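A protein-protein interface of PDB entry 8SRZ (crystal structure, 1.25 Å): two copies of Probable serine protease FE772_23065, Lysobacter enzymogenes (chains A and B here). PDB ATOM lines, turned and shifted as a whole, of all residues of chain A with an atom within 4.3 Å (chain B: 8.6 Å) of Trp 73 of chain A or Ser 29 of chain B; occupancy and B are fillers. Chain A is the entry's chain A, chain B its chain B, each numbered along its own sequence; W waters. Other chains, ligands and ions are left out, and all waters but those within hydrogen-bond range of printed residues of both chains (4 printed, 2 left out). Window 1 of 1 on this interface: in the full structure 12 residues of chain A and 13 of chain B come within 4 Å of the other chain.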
ATOM      1  N   LEU A  18      14.029  33.738   4.104  1.00  0.00           N
ATOM      2  CA  LEU A  18      15.431  33.607   4.397  1.00  0.00           C
ATOM      3  C   LEU A  18      16.279  34.256   3.326  1.00  0.00           C
ATOM      4  O   LEU A  18      15.862  34.389   2.159  1.00  0.00           O
ATOM      5  CB  LEU A  18      15.784  32.129   4.471  1.00  0.00           C
ATOM      6  CG  LEU A  18      15.086  31.338   5.581  1.00  0.00           C
ATOM      7  CD1 LEU A  18      15.530  29.878   5.551  1.00  0.00           C
ATOM      8  CD2 LEU A  18      15.391  31.875   6.919  1.00  0.00           C
ATOM      9  N   CYS A  26      21.148  25.581   3.963  1.00  0.00           N
ATOM     10  CA  CYS A  26      20.225  24.445   4.008  1.00  0.00           C
ATOM     11  C   CYS A  26      20.482  23.493   2.846  1.00  0.00           C
ATOM     12  O   CYS A  26      20.424  22.299   3.000  1.00  0.00           O
ATOM     13  CB  CYS A  26      18.808  25.000   3.952  1.00  0.00           C
ATOM     14  SG  CYS A  26      18.266  25.959   5.373  1.00  0.00           S
ATOM     15  N   SER A  29      23.342  21.141   3.282  1.00  0.00           N
ATOM     16  CA  SER A  29      23.055  20.002   4.159  1.00  0.00           C
ATOM     17  C   SER A  29      22.224  18.949   3.494  1.00  0.00           C
ATOM     18  O   SER A  29      22.465  17.733   3.676  1.00  0.00           O
ATOM     19  CB  SER A  29      22.345  20.485   5.409  1.00  0.00           C
ATOM     20  OG  SER A  29      23.297  21.100   6.276  1.00  0.00           O
ATOM     21  N   ALA A  69      13.864  21.856   5.835  1.00  0.00           N
ATOM     22  CA  ALA A  69      14.993  22.596   6.377  1.00  0.00           C
ATOM     23  C   ALA A  69      14.682  24.082   6.476  1.00  0.00           C
ATOM     24  O   ALA A  69      14.906  24.719   7.506  1.00  0.00           O
ATOM     25  CB  ALA A  69      16.230  22.380   5.529  1.00  0.00           C
ATOM     26  N   ILE A  70      14.156  24.676   5.393  1.00  0.00           N
ATOM     27  CA  ILE A  70      13.828  26.089   5.407  1.00  0.00           C
ATOM     28  C   ILE A  70      12.776  26.386   6.444  1.00  0.00           C
ATOM     29  O   ILE A  70      12.871  27.362   7.191  1.00  0.00           O
ATOM     30  CB  ILE A  70      13.430  26.528   3.979  1.00  0.00           C
ATOM     31  CG1 ILE A  70      14.703  26.620   3.102  1.00  0.00           C
ATOM     32  CG2 ILE A  70      12.658  27.856   3.968  1.00  0.00           C
ATOM     33  CD1 ILE A  70      14.428  26.697   1.657  1.00  0.00           C
ATOM     34  N   GLY A  71      11.744  25.545   6.534  1.00  0.00           N
ATOM     35  CA  GLY A  71      10.739  25.722   7.564  1.00  0.00           C
ATOM     36  C   GLY A  71      11.302  25.679   8.961  1.00  0.00           C
ATOM     37  O   GLY A  71      10.896  26.415   9.846  1.00  0.00           O
ATOM     38  N   ASN A  72      12.264  24.768   9.188  1.00  0.00           N
ATOM     39  CA  ASN A  72      12.884  24.645  10.506  1.00  0.00           C
ATOM     40  C   ASN A  72      13.627  25.928  10.878  1.00  0.00           C
ATOM     41  O   ASN A  72      13.555  26.364  12.051  1.00  0.00           O
ATOM     42  CB  ASN A  72      13.838  23.459  10.497  1.00  0.00           C
ATOM     43  CG  ASN A  72      13.176  22.111  10.684  1.00  0.00           C
ATOM     44  OD1 ASN A  72      12.016  22.034  11.139  1.00  0.00           O
ATOM     45  ND2 ASN A  72      13.856  21.058  10.350  1.00  0.00           N
ATOM     46  N   TRP A  73      14.341  26.510   9.949  1.00  0.00           N
ATOM     47  CA  TRP A  73      15.053  27.786  10.208  1.00  0.00           C
ATOM     48  C   TRP A  73      14.107  28.979  10.307  1.00  0.00           C
ATOM     49  O   TRP A  73      14.275  29.839  11.195  1.00  0.00           O
ATOM     50  CB  TRP A  73      16.129  28.033   9.205  1.00  0.00           C
ATOM     51  CG  TRP A  73      17.308  27.141   9.401  1.00  0.00           C
ATOM     52  CD1 TRP A  73      17.571  26.026   8.744  1.00  0.00           C
ATOM     53  CD2 TRP A  73      18.344  27.275  10.398  1.00  0.00           C
ATOM     54  NE1 TRP A  73      18.742  25.443   9.193  1.00  0.00           N
ATOM     55  CE2 TRP A  73      19.232  26.215  10.210  1.00  0.00           C
ATOM     56  CE3 TRP A  73      18.582  28.130  11.468  1.00  0.00           C
ATOM     57  CZ2 TRP A  73      20.395  26.030  10.978  1.00  0.00           C
ATOM     58  CZ3 TRP A  73      19.732  27.944  12.238  1.00  0.00           C
ATOM     59  CH2 TRP A  73      20.613  26.914  11.963  1.00  0.00           C
ATOM     60  N   GLU A  74      13.002  28.949   9.587  1.00  0.00           N
ATOM     61  CA  GLU A  74      11.968  29.975   9.738  1.00  0.00           C
ATOM     62  C   GLU A  74      11.337  29.875  11.079  1.00  0.00           C
ATOM     63  O   GLU A  74      11.027  30.904  11.705  1.00  0.00           O
ATOM     64  CB  GLU A  74      10.944  29.853   8.617  1.00  0.00           C
ATOM     65  CG  GLU A  74      11.548  30.207   7.245  1.00  0.00           C
ATOM     66  CD  GLU A  74      10.995  31.399   6.492  1.00  0.00           C
ATOM     67  OE1 GLU A  74      10.325  32.247   7.069  1.00  0.00           O
ATOM     68  OE2 GLU A  74      11.402  31.465   5.289  1.00  0.00           O
ATOM     69  N   GLN A  75      11.057  28.675  11.553  1.00  0.00           N
ATOM     70  CA  GLN A  75      10.517  28.475  12.894  1.00  0.00           C
ATOM     71  C   GLN A  75      11.461  29.064  13.951  1.00  0.00           C
ATOM     72  O   GLN A  75      10.996  29.752  14.888  1.00  0.00           O
ATOM     73  CB  GLN A  75      10.262  26.976  13.093  1.00  0.00           C
ATOM     74  CG  GLN A  75       9.833  26.564  14.476  1.00  0.00           C
ATOM     75  CD  GLN A  75       9.589  25.044  14.438  1.00  0.00           C
ATOM     76  OE1 GLN A  75      10.556  24.273  14.423  1.00  0.00           O
ATOM     77  NE2 GLN A  75       8.321  24.619  14.298  1.00  0.00           N
ATOM     78  N   LYS A  76      12.764  28.946  13.757  1.00  0.00           N
ATOM     79  CA  LYS A  76      13.675  29.612  14.704  1.00  0.00           C
ATOM     80  C   LYS A  76      13.627  31.130  14.619  1.00  0.00           C
ATOM     81  O   LYS A  76      13.940  31.811  15.615  1.00  0.00           O
ATOM     82  CB  LYS A  76      15.067  29.099  14.465  1.00  0.00           C
ATOM     83  CG  LYS A  76      15.088  27.690  14.924  1.00  0.00           C
ATOM     84  CD  LYS A  76      16.435  27.006  14.531  1.00  0.00           C
ATOM     85  CE  LYS A  76      17.608  27.555  15.266  1.00  0.00           C
ATOM     86  NZ  LYS A  76      17.682  27.052  16.692  1.00  0.00           N
ATOM     87  N   ALA A  77      13.295  31.694  13.463  1.00  0.00           N
ATOM     88  CA  ALA A  77      13.071  33.121  13.280  1.00  0.00           C
ATOM     89  C   ALA A  77      11.683  33.534  13.702  1.00  0.00           C
ATOM     90  O   ALA A  77      11.363  34.688  13.416  1.00  0.00           O
ATOM     91  CB  ALA A  77      13.404  33.514  11.824  1.00  0.00           C
ATOM     92  N   GLU B  21      28.896  23.792  16.523  1.00  0.00           N
ATOM     93  CA  GLU B  21      28.041  24.762  15.828  1.00  0.00           C
ATOM     94  C   GLU B  21      27.581  24.182  14.512  1.00  0.00           C
ATOM     95  O   GLU B  21      26.380  24.246  14.179  1.00  0.00           O
ATOM     96  CB  GLU B  21      28.774  26.086  15.593  1.00  0.00           C
ATOM     97  CG  GLU B  21      27.959  27.181  14.929  1.00  0.00           C
ATOM     98  CD  GLU B  21      28.817  28.331  14.430  1.00  0.00           C
ATOM     99  OE1 GLU B  21      30.054  28.209  14.373  1.00  0.00           O
ATOM    100  OE2 GLU B  21      28.256  29.367  14.047  1.00  0.00           O
ATOM    101  N   PHE B  22      28.501  23.652  13.716  1.00  0.00           N
ATOM    102  CA  PHE B  22      28.118  23.136  12.409  1.00  0.00           C
ATOM    103  C   PHE B  22      27.262  21.908  12.527  1.00  0.00           C
ATOM    104  O   PHE B  22      26.345  21.683  11.746  1.00  0.00           O
ATOM    105  CB  PHE B  22      29.355  22.828  11.561  1.00  0.00           C
ATOM    106  CG  PHE B  22      29.914  24.053  10.863  1.00  0.00           C
ATOM    107  CD1 PHE B  22      29.892  25.299  11.501  1.00  0.00           C
ATOM    108  CD2 PHE B  22      30.495  23.966   9.615  1.00  0.00           C
ATOM    109  CE1 PHE B  22      30.413  26.471  10.824  1.00  0.00           C
ATOM    110  CE2 PHE B  22      31.020  25.116   8.936  1.00  0.00           C
ATOM    111  CZ  PHE B  22      30.998  26.321   9.540  1.00  0.00           C
ATOM    112  N   ILE B  23      27.560  21.029  13.497  1.00  0.00           N
ATOM    113  CA  ILE B  23      26.743  19.838  13.691  1.00  0.00           C
ATOM    114  C   ILE B  23      25.333  20.222  14.076  1.00  0.00           C
ATOM    115  O   ILE B  23      24.367  19.667  13.540  1.00  0.00           O
ATOM    116  CB  ILE B  23      27.385  18.910  14.757  1.00  0.00           C
ATOM    117  CG1 ILE B  23      28.707  18.347  14.222  1.00  0.00           C
ATOM    118  CG2 ILE B  23      26.432  17.798  15.198  1.00  0.00           C
ATOM    119  CD1 ILE B  23      29.590  17.660  15.269  1.00  0.00           C
ATOM    120  N   GLY B  24      25.185  21.188  14.973  1.00  0.00           N
ATOM    121  CA  GLY B  24      23.880  21.644  15.359  1.00  0.00           C
ATOM    122  C   GLY B  24      23.129  22.230  14.195  1.00  0.00           C
ATOM    123  O   GLY B  24      21.902  22.060  14.060  1.00  0.00           O
ATOM    124  N   ASN B  25      23.813  22.986  13.362  1.00  0.00           N
ATOM    125  CA  ASN B  25      23.157  23.584  12.199  1.00  0.00           C
ATOM    126  C   ASN B  25      22.661  22.483  11.268  1.00  0.00           C
ATOM    127  O   ASN B  25      21.502  22.607  10.742  1.00  0.00           O
ATOM    128  CB  ASN B  25      24.135  24.492  11.498  1.00  0.00           C
ATOM    129  CG  ASN B  25      24.384  25.767  12.209  1.00  0.00           C
ATOM    130  OD1 ASN B  25      23.765  26.142  13.193  1.00  0.00           O
ATOM    131  ND2 ASN B  25      25.363  26.451  11.685  1.00  0.00           N
ATOM    132  N   CYS B  26      23.425  21.458  10.997  1.00  0.00           N
ATOM    133  CA  CYS B  26      22.966  20.339  10.213  1.00  0.00           C
ATOM    134  C   CYS B  26      21.742  19.700  10.836  1.00  0.00           C
ATOM    135  O   CYS B  26      20.788  19.329  10.131  1.00  0.00           O
ATOM    136  CB  CYS B  26      24.103  19.327  10.074  1.00  0.00           C
ATOM    137  SG  CYS B  26      25.467  19.810   9.048  1.00  0.00           S
ATOM    138  N   TYR B  27      21.765  19.477  12.140  1.00  0.00           N
ATOM    139  CA  TYR B  27      20.639  18.873  12.829  1.00  0.00           C
ATOM    140  C   TYR B  27      19.384  19.724  12.619  1.00  0.00           C
ATOM    141  O   TYR B  27      18.316  19.177  12.325  1.00  0.00           O
ATOM    142  CB  TYR B  27      20.949  18.690  14.320  1.00  0.00           C
ATOM    143  CG  TYR B  27      19.875  17.992  15.101  1.00  0.00           C
ATOM    144  CD1 TYR B  27      18.723  18.660  15.550  1.00  0.00           C
ATOM    145  CD2 TYR B  27      19.971  16.649  15.396  1.00  0.00           C
ATOM    146  CE1 TYR B  27      17.730  17.993  16.254  1.00  0.00           C
ATOM    147  CE2 TYR B  27      19.019  15.997  16.161  1.00  0.00           C
ATOM    148  CZ  TYR B  27      17.872  16.653  16.553  1.00  0.00           C
ATOM    149  OH  TYR B  27      16.932  15.951  17.227  1.00  0.00           O
ATOM    150  N   VAL B  28      19.518  21.034  12.794  1.00  0.00           N
ATOM    151  CA  VAL B  28      18.356  21.912  12.620  1.00  0.00           C
ATOM    152  C   VAL B  28      17.759  21.751  11.231  1.00  0.00           C
ATOM    153  O   VAL B  28      16.517  21.709  11.083  1.00  0.00           O
ATOM    154  CB  VAL B  28      18.723  23.374  12.911  1.00  0.00           C
ATOM    155  CG1 VAL B  28      17.597  24.317  12.426  1.00  0.00           C
ATOM    156  CG2 VAL B  28      19.061  23.587  14.364  1.00  0.00           C
ATOM    157  N   SER B  29      18.607  21.678  10.201  1.00  0.00           N
ATOM    158  CA  SER B  29      18.098  21.554   8.849  1.00  0.00           C
ATOM    159  C   SER B  29      17.408  20.236   8.632  1.00  0.00           C
ATOM    160  O   SER B  29      16.383  20.161   7.949  1.00  0.00           O
ATOM    161  CB  SER B  29      19.220  21.704   7.853  1.00  0.00           C
ATOM    162  OG  SER B  29      19.595  23.084   7.771  1.00  0.00           O
ATOM    163  N   VAL B  30      17.996  19.131   9.098  1.00  0.00           N
ATOM    164  CA  VAL B  30      17.504  17.825   8.695  1.00  0.00           C
ATOM    165  C   VAL B  30      16.437  17.258   9.620  1.00  0.00           C
ATOM    166  O   VAL B  30      15.746  16.311   9.246  1.00  0.00           O
ATOM    167  CB  VAL B  30      18.622  16.773   8.561  1.00  0.00           C
ATOM    168  CG1 VAL B  30      19.599  17.160   7.495  1.00  0.00           C
ATOM    169  CG2 VAL B  30      19.277  16.431   9.808  1.00  0.00           C
ATOM    170  N   ARG B  31      16.241  17.825  10.768  1.00  0.00           N
ATOM    171  CA  ARG B  31      15.304  17.373  11.811  1.00  0.00           C
ATOM    172  C   ARG B  31      13.890  17.181  11.282  1.00  0.00           C
ATOM    173  O   ARG B  31      13.302  18.179  10.916  1.00  0.00           O
ATOM    174  CB  ARG B  31      15.251  18.514  12.988  1.00  0.00           C
ATOM    175  CG  ARG B  31      14.291  18.016  14.156  1.00  0.00           C
ATOM    176  CD  ARG B  31      14.075  19.012  15.059  1.00  0.00           C
ATOM    177  NE  ARG B  31      13.287  20.060  14.473  1.00  0.00           N
ATOM    178  CZ  ARG B  31      12.027  20.183  14.736  1.00  0.00           C
ATOM    179  NH1 ARG B  31      11.327  19.261  15.356  1.00  0.00           N
ATOM    180  NH2 ARG B  31      11.424  21.311  14.394  1.00  0.00           N
ATOM    181  N   PRO B  32      13.259  16.011  11.356  1.00  0.00           N
ATOM    182  CA  PRO B  32      11.827  15.886  11.063  1.00  0.00           C
ATOM    183  C   PRO B  32      11.021  16.254  12.281  1.00  0.00           C
ATOM    184  O   PRO B  32      11.525  16.374  13.402  1.00  0.00           O
ATOM    185  CB  PRO B  32      11.698  14.406  10.716  1.00  0.00           C
ATOM    186  CG  PRO B  32      12.698  13.758  11.639  1.00  0.00           C
ATOM    187  CD  PRO B  32      13.866  14.701  11.669  1.00  0.00           C
ATOM    188  N   TRP B  38      16.780  21.059  18.440  1.00  0.00           N
ATOM    189  CA  TRP B  38      18.162  21.143  18.866  1.00  0.00           C
ATOM    190  C   TRP B  38      18.279  21.582  20.312  1.00  0.00           C
ATOM    191  O   TRP B  38      19.045  21.012  21.055  1.00  0.00           O
ATOM    192  CB  TRP B  38      18.907  22.060  17.916  1.00  0.00           C
ATOM    193  CG  TRP B  38      20.354  22.246  18.280  1.00  0.00           C
ATOM    194  CD1 TRP B  38      20.924  23.364  18.802  1.00  0.00           C
ATOM    195  CD2 TRP B  38      21.360  21.256  18.268  1.00  0.00           C
ATOM    196  NE1 TRP B  38      22.253  23.169  19.030  1.00  0.00           N
ATOM    197  CE2 TRP B  38      22.532  21.884  18.681  1.00  0.00           C
ATOM    198  CE3 TRP B  38      21.398  19.935  17.884  1.00  0.00           C
ATOM    199  CZ2 TRP B  38      23.727  21.203  18.791  1.00  0.00           C
ATOM    200  CZ3 TRP B  38      22.630  19.302  17.937  1.00  0.00           C
ATOM    201  CH2 TRP B  38      23.745  19.939  18.421  1.00  0.00           C
ATOM    202  N   GLU B  39      17.451  22.568  20.762  1.00  0.00           N
ATOM    203  CA  GLU B  39      17.609  23.098  22.131  1.00  0.00           C
ATOM    204  C   GLU B  39      17.249  22.044  23.164  1.00  0.00           C
ATOM    205  O   GLU B  39      17.828  21.974  24.274  1.00  0.00           O
ATOM    206  CB  GLU B  39      16.690  24.317  22.342  1.00  0.00           C
ATOM    207  CG  GLU B  39      17.127  25.568  21.576  1.00  0.00           C
ATOM    208  CD  GLU B  39      16.950  25.465  20.076  1.00  0.00           C
ATOM    209  OE1 GLU B  39      16.069  24.668  19.642  1.00  0.00           O
ATOM    210  OE2 GLU B  39      17.721  26.157  19.340  1.00  0.00           O
ATOM    211  N   PHE B  62      16.550   9.330  11.177  1.00  0.00           N
ATOM    212  CA  PHE B  62      17.127  10.263  10.224  1.00  0.00           C
ATOM    213  C   PHE B  62      18.645  10.345  10.334  1.00  0.00           C
ATOM    214  O   PHE B  62      19.204  11.300   9.851  1.00  0.00           O
ATOM    215  CB  PHE B  62      16.471  11.662  10.303  1.00  0.00           C
ATOM    216  CG  PHE B  62      16.722  12.440  11.583  1.00  0.00           C
ATOM    217  CD1 PHE B  62      15.951  12.191  12.711  1.00  0.00           C
ATOM    218  CD2 PHE B  62      17.628  13.509  11.602  1.00  0.00           C
ATOM    219  CE1 PHE B  62      16.116  12.959  13.875  1.00  0.00           C
ATOM    220  CE2 PHE B  62      17.805  14.265  12.737  1.00  0.00           C
ATOM    221  CZ  PHE B  62      17.033  13.994  13.893  1.00  0.00           C
ATOM    222  N   ARG B  65      20.230  10.784   6.911  1.00  0.00           N
ATOM    223  CA  ARG B  65      20.218  12.139   6.356  1.00  0.00           C
ATOM    224  C   ARG B  65      21.177  13.044   7.076  1.00  0.00           C
ATOM    225  O   ARG B  65      21.781  13.930   6.452  1.00  0.00           O
ATOM    226  CB  ARG B  65      18.770  12.662   6.351  1.00  0.00           C
ATOM    227  CG  ARG B  65      17.974  11.957   5.139  1.00  0.00           C
ATOM    228  CD  ARG B  65      16.634  12.603   4.860  1.00  0.00           C
ATOM    229  NE  ARG B  65      15.896  12.899   6.066  1.00  0.00           N
ATOM    230  CZ  ARG B  65      15.782  14.095   6.628  1.00  0.00           C
ATOM    231  NH1 ARG B  65      16.206  15.247   6.007  1.00  0.00           N
ATOM    232  NH2 ARG B  65      15.120  14.160   7.773  1.00  0.00           N
ATOM    233  N   LEU B  66      21.272  12.894   8.401  1.00  0.00           N
ATOM    234  CA  LEU B  66      22.201  13.700   9.126  1.00  0.00           C
ATOM    235  C   LEU B  66      23.631  13.361   8.724  1.00  0.00           C
ATOM    236  O   LEU B  66      24.453  14.255   8.604  1.00  0.00           O
ATOM    237  CB  LEU B  66      21.953  13.567  10.643  1.00  0.00           C
ATOM    238  CG  LEU B  66      22.804  14.418  11.564  1.00  0.00           C
ATOM    239  CD1 LEU B  66      22.836  15.869  11.106  1.00  0.00           C
ATOM    240  CD2 LEU B  66      22.266  14.267  12.988  1.00  0.00           C
ATOM    241  N   ALA B  69      24.406  15.159   5.551  1.00  0.00           N
ATOM    242  CA  ALA B  69      24.642  16.573   5.791  1.00  0.00           C
ATOM    243  C   ALA B  69      26.045  16.795   6.338  1.00  0.00           C
ATOM    244  O   ALA B  69      26.758  17.701   5.921  1.00  0.00           O
ATOM    245  CB  ALA B  69      23.603  17.126   6.780  1.00  0.00           C
ATOM    246  N   TRP B  73      29.233  19.016   4.626  1.00  0.00           N
ATOM    247  CA  TRP B  73      30.018  20.114   5.205  1.00  0.00           C
ATOM    248  C   TRP B  73      31.481  19.722   5.317  1.00  0.00           C
ATOM    249  O   TRP B  73      32.384  20.534   5.114  1.00  0.00           O
ATOM    250  CB  TRP B  73      29.427  20.553   6.553  1.00  0.00           C
ATOM    251  CG  TRP B  73      28.162  21.359   6.308  1.00  0.00           C
ATOM    252  CD1 TRP B  73      26.918  20.908   6.242  1.00  0.00           C
ATOM    253  CD2 TRP B  73      28.079  22.754   6.014  1.00  0.00           C
ATOM    254  NE1 TRP B  73      26.044  21.909   5.904  1.00  0.00           N
ATOM    255  CE2 TRP B  73      26.741  23.049   5.740  1.00  0.00           C
ATOM    256  CE3 TRP B  73      29.045  23.751   5.914  1.00  0.00           C
ATOM    257  CZ2 TRP B  73      26.291  24.322   5.434  1.00  0.00           C
ATOM    258  CZ3 TRP B  73      28.589  25.040   5.626  1.00  0.00           C
ATOM    259  CH2 TRP B  73      27.224  25.282   5.341  1.00  0.00           C
HETATM  260  O   HOH W   1      21.030  15.310   4.087  1.00  0.00           O
HETATM  261  O   HOH W   2      10.834  19.499  11.263  1.00  0.00           O
HETATM  262  O   HOH W   3      14.893  22.136  13.458  1.00  0.00           O
HETATM  263  O   HOH W   4       8.564  21.796  14.685  1.00  0.00           O
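Water W2 bridges OD1 of Asn 72 of chain A (2.8 Å) and O of Arg 31 of chain B (2.8 Å). Water W3 lies within hydrogen-bond range of NE of Arg 31 of chain B (2.8 Å), O of Val 28 of chain B (2.9 Å) and ND2 of Asn 72 of chain A (3.4 Å). Water W1 lies within hydrogen-bond range of the backbone carbonyl oxygen of Arg 65 of chain B (2.8 Å) and the backbone carbonyl oxygen of Ser 29 of chain A (2.8 Å). Water W4 lies within hydrogen-bond range of NE2 of Gln 75 of chain A (2.9 Å) and NH2 of Arg 31 of chain B (2.9 Å).
Among the printed residues, merely in contact across the chains: Ala 69 of chain A with Ser 29 of chain B, Ser 29 of chain A with Ala 69 of chain B, Trp 73 of chain A with Val 28 of chain B, Trp 73 of chain A with Asn 25 of chain B, Asn 72 of chain A with Ser 29 of chain B, Lys 76 of chain A with Val 28 of chain B and Cys 26 of chain A with Ser 29 of chain B.
Cys 26 of chain A touches Ser 29 of chain B, and with the chains exchanged Ser 29 of chain A touches Cys 26 of chain B. Ser 29 of chain A touches Ala 69 of chain B, and with the chains exchanged Ala 69 of chain A touches Ser 29 of chain B. Ser 29 of chain A touches Trp 73 of chain B, and with the chains exchanged Trp 73 of chain A touches Ser 29 of chain B. 4 positions are printed for both chains. Of the 14 pairs that touch across the chains among the printed residues, 6 have their exchanged pair printed and touching as well.
The backbone carbonyl oxygen (O) of Glu 21 of chain B sits close to the side-chain amide oxygen (OD1) of Asn 25 of chain B (3.4 Å). The side-chain sulfur (SG) of Cys 26 of chain B sits at hydrogen-bond distance from the backbone carbonyl oxygen (O) of Phe 22 of chain B.
The side-chain sulfur (SG) of Cys 26 of chain B lies within hydrogen-bond range of the side-chain hydroxyl (OG) of Ser 29 of chain A (3.7 Å). NE1 of Trp 73 of chain B is in hydrogen-bond range of OG of Ser 29 of chain A. ND2 of Asn 72 of chain A is in hydrogen-bond range of O of Val 28 of chain B (2.8 Å). ND2 of Asn 72 of chain A is in hydrogen-bond range of O of Arg 31 of chain B. The side-chain hydroxyl (OG) of Ser 29 of chain B is in hydrogen-bond range of the indole nitrogen (NE1) of Trp 73 of chain A (2.9 Å). OE1 of Gln 75 of chain A is in hydrogen-bond range of NH2 of Arg 31 of chain B (3.1 Å). The side-chain carboxylate (OE2) of Glu 39 of chain B is in salt-bridge range of the side-chain amino group (NZ) of Lys 76 of chain A, 2.8 Å away.
Of the 19 printed residues of chain B, 8 touch a printed residue of chain A. Printed residues of chain B that touch a printed residue of chain A: Asn 25, Cys 26, Val 28, Ser 29, Arg 31, Glu 39, Ala 69 and Trp 73. Hydrophobic or aromatic side chains of chain B within 4 Å of the printed part of chain A: Val 28, Ala 69 and Trp 73. Of the 12 printed residues of chain A, 7 touch a printed residue of chain B. Printed residues of chain A that touch a printed residue of chain B: Cys 26, Ser 29, Ala 69, Asn 72, Trp 73, Gln 75 and Lys 76. Among the printed residues, 14 pairs touch across the chains. Among the printed residues, Asp or Glu carboxylates within 4 Å of a Lys or Arg side-chain nitrogen of the other chain: Lys 76 of chain A with Glu 39 of chain B.
Trp 73 of chain A touches just these residues of chain B: Asn 25 (3.5 Å), Val 28 (3.3 Å) and Ser 29 (2.9 Å). Of the printed residues of chain A, Ser 29 of chain B touches Cys 26, Ala 69, Asn 72 and Trp 73. Ala 69 of chain A touches just one residue of chain B: Ser 29 (3.2 Å). No residue of chain B comes within 4 Å of Gly 71 of chain A. Printed residues of chain A within 4 Å of Trp 73 of chain B: Ser 29 (2.9 Å). Of the printed residues of chain B, Cys 26 of chain A touches Ser 29. Of the printed residues of chain A, Cys 26 of chain B touches Ser 29 (3.7 Å). Of the printed residues of chain A, Ala 69 of chain B touches Ser 29. Ile 23 of chain B touches none of the printed residues of chain A. The nearest residue of chain B that does not touch Trp 73 of chain A is Gly 24 of chain B (5.2 Å).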
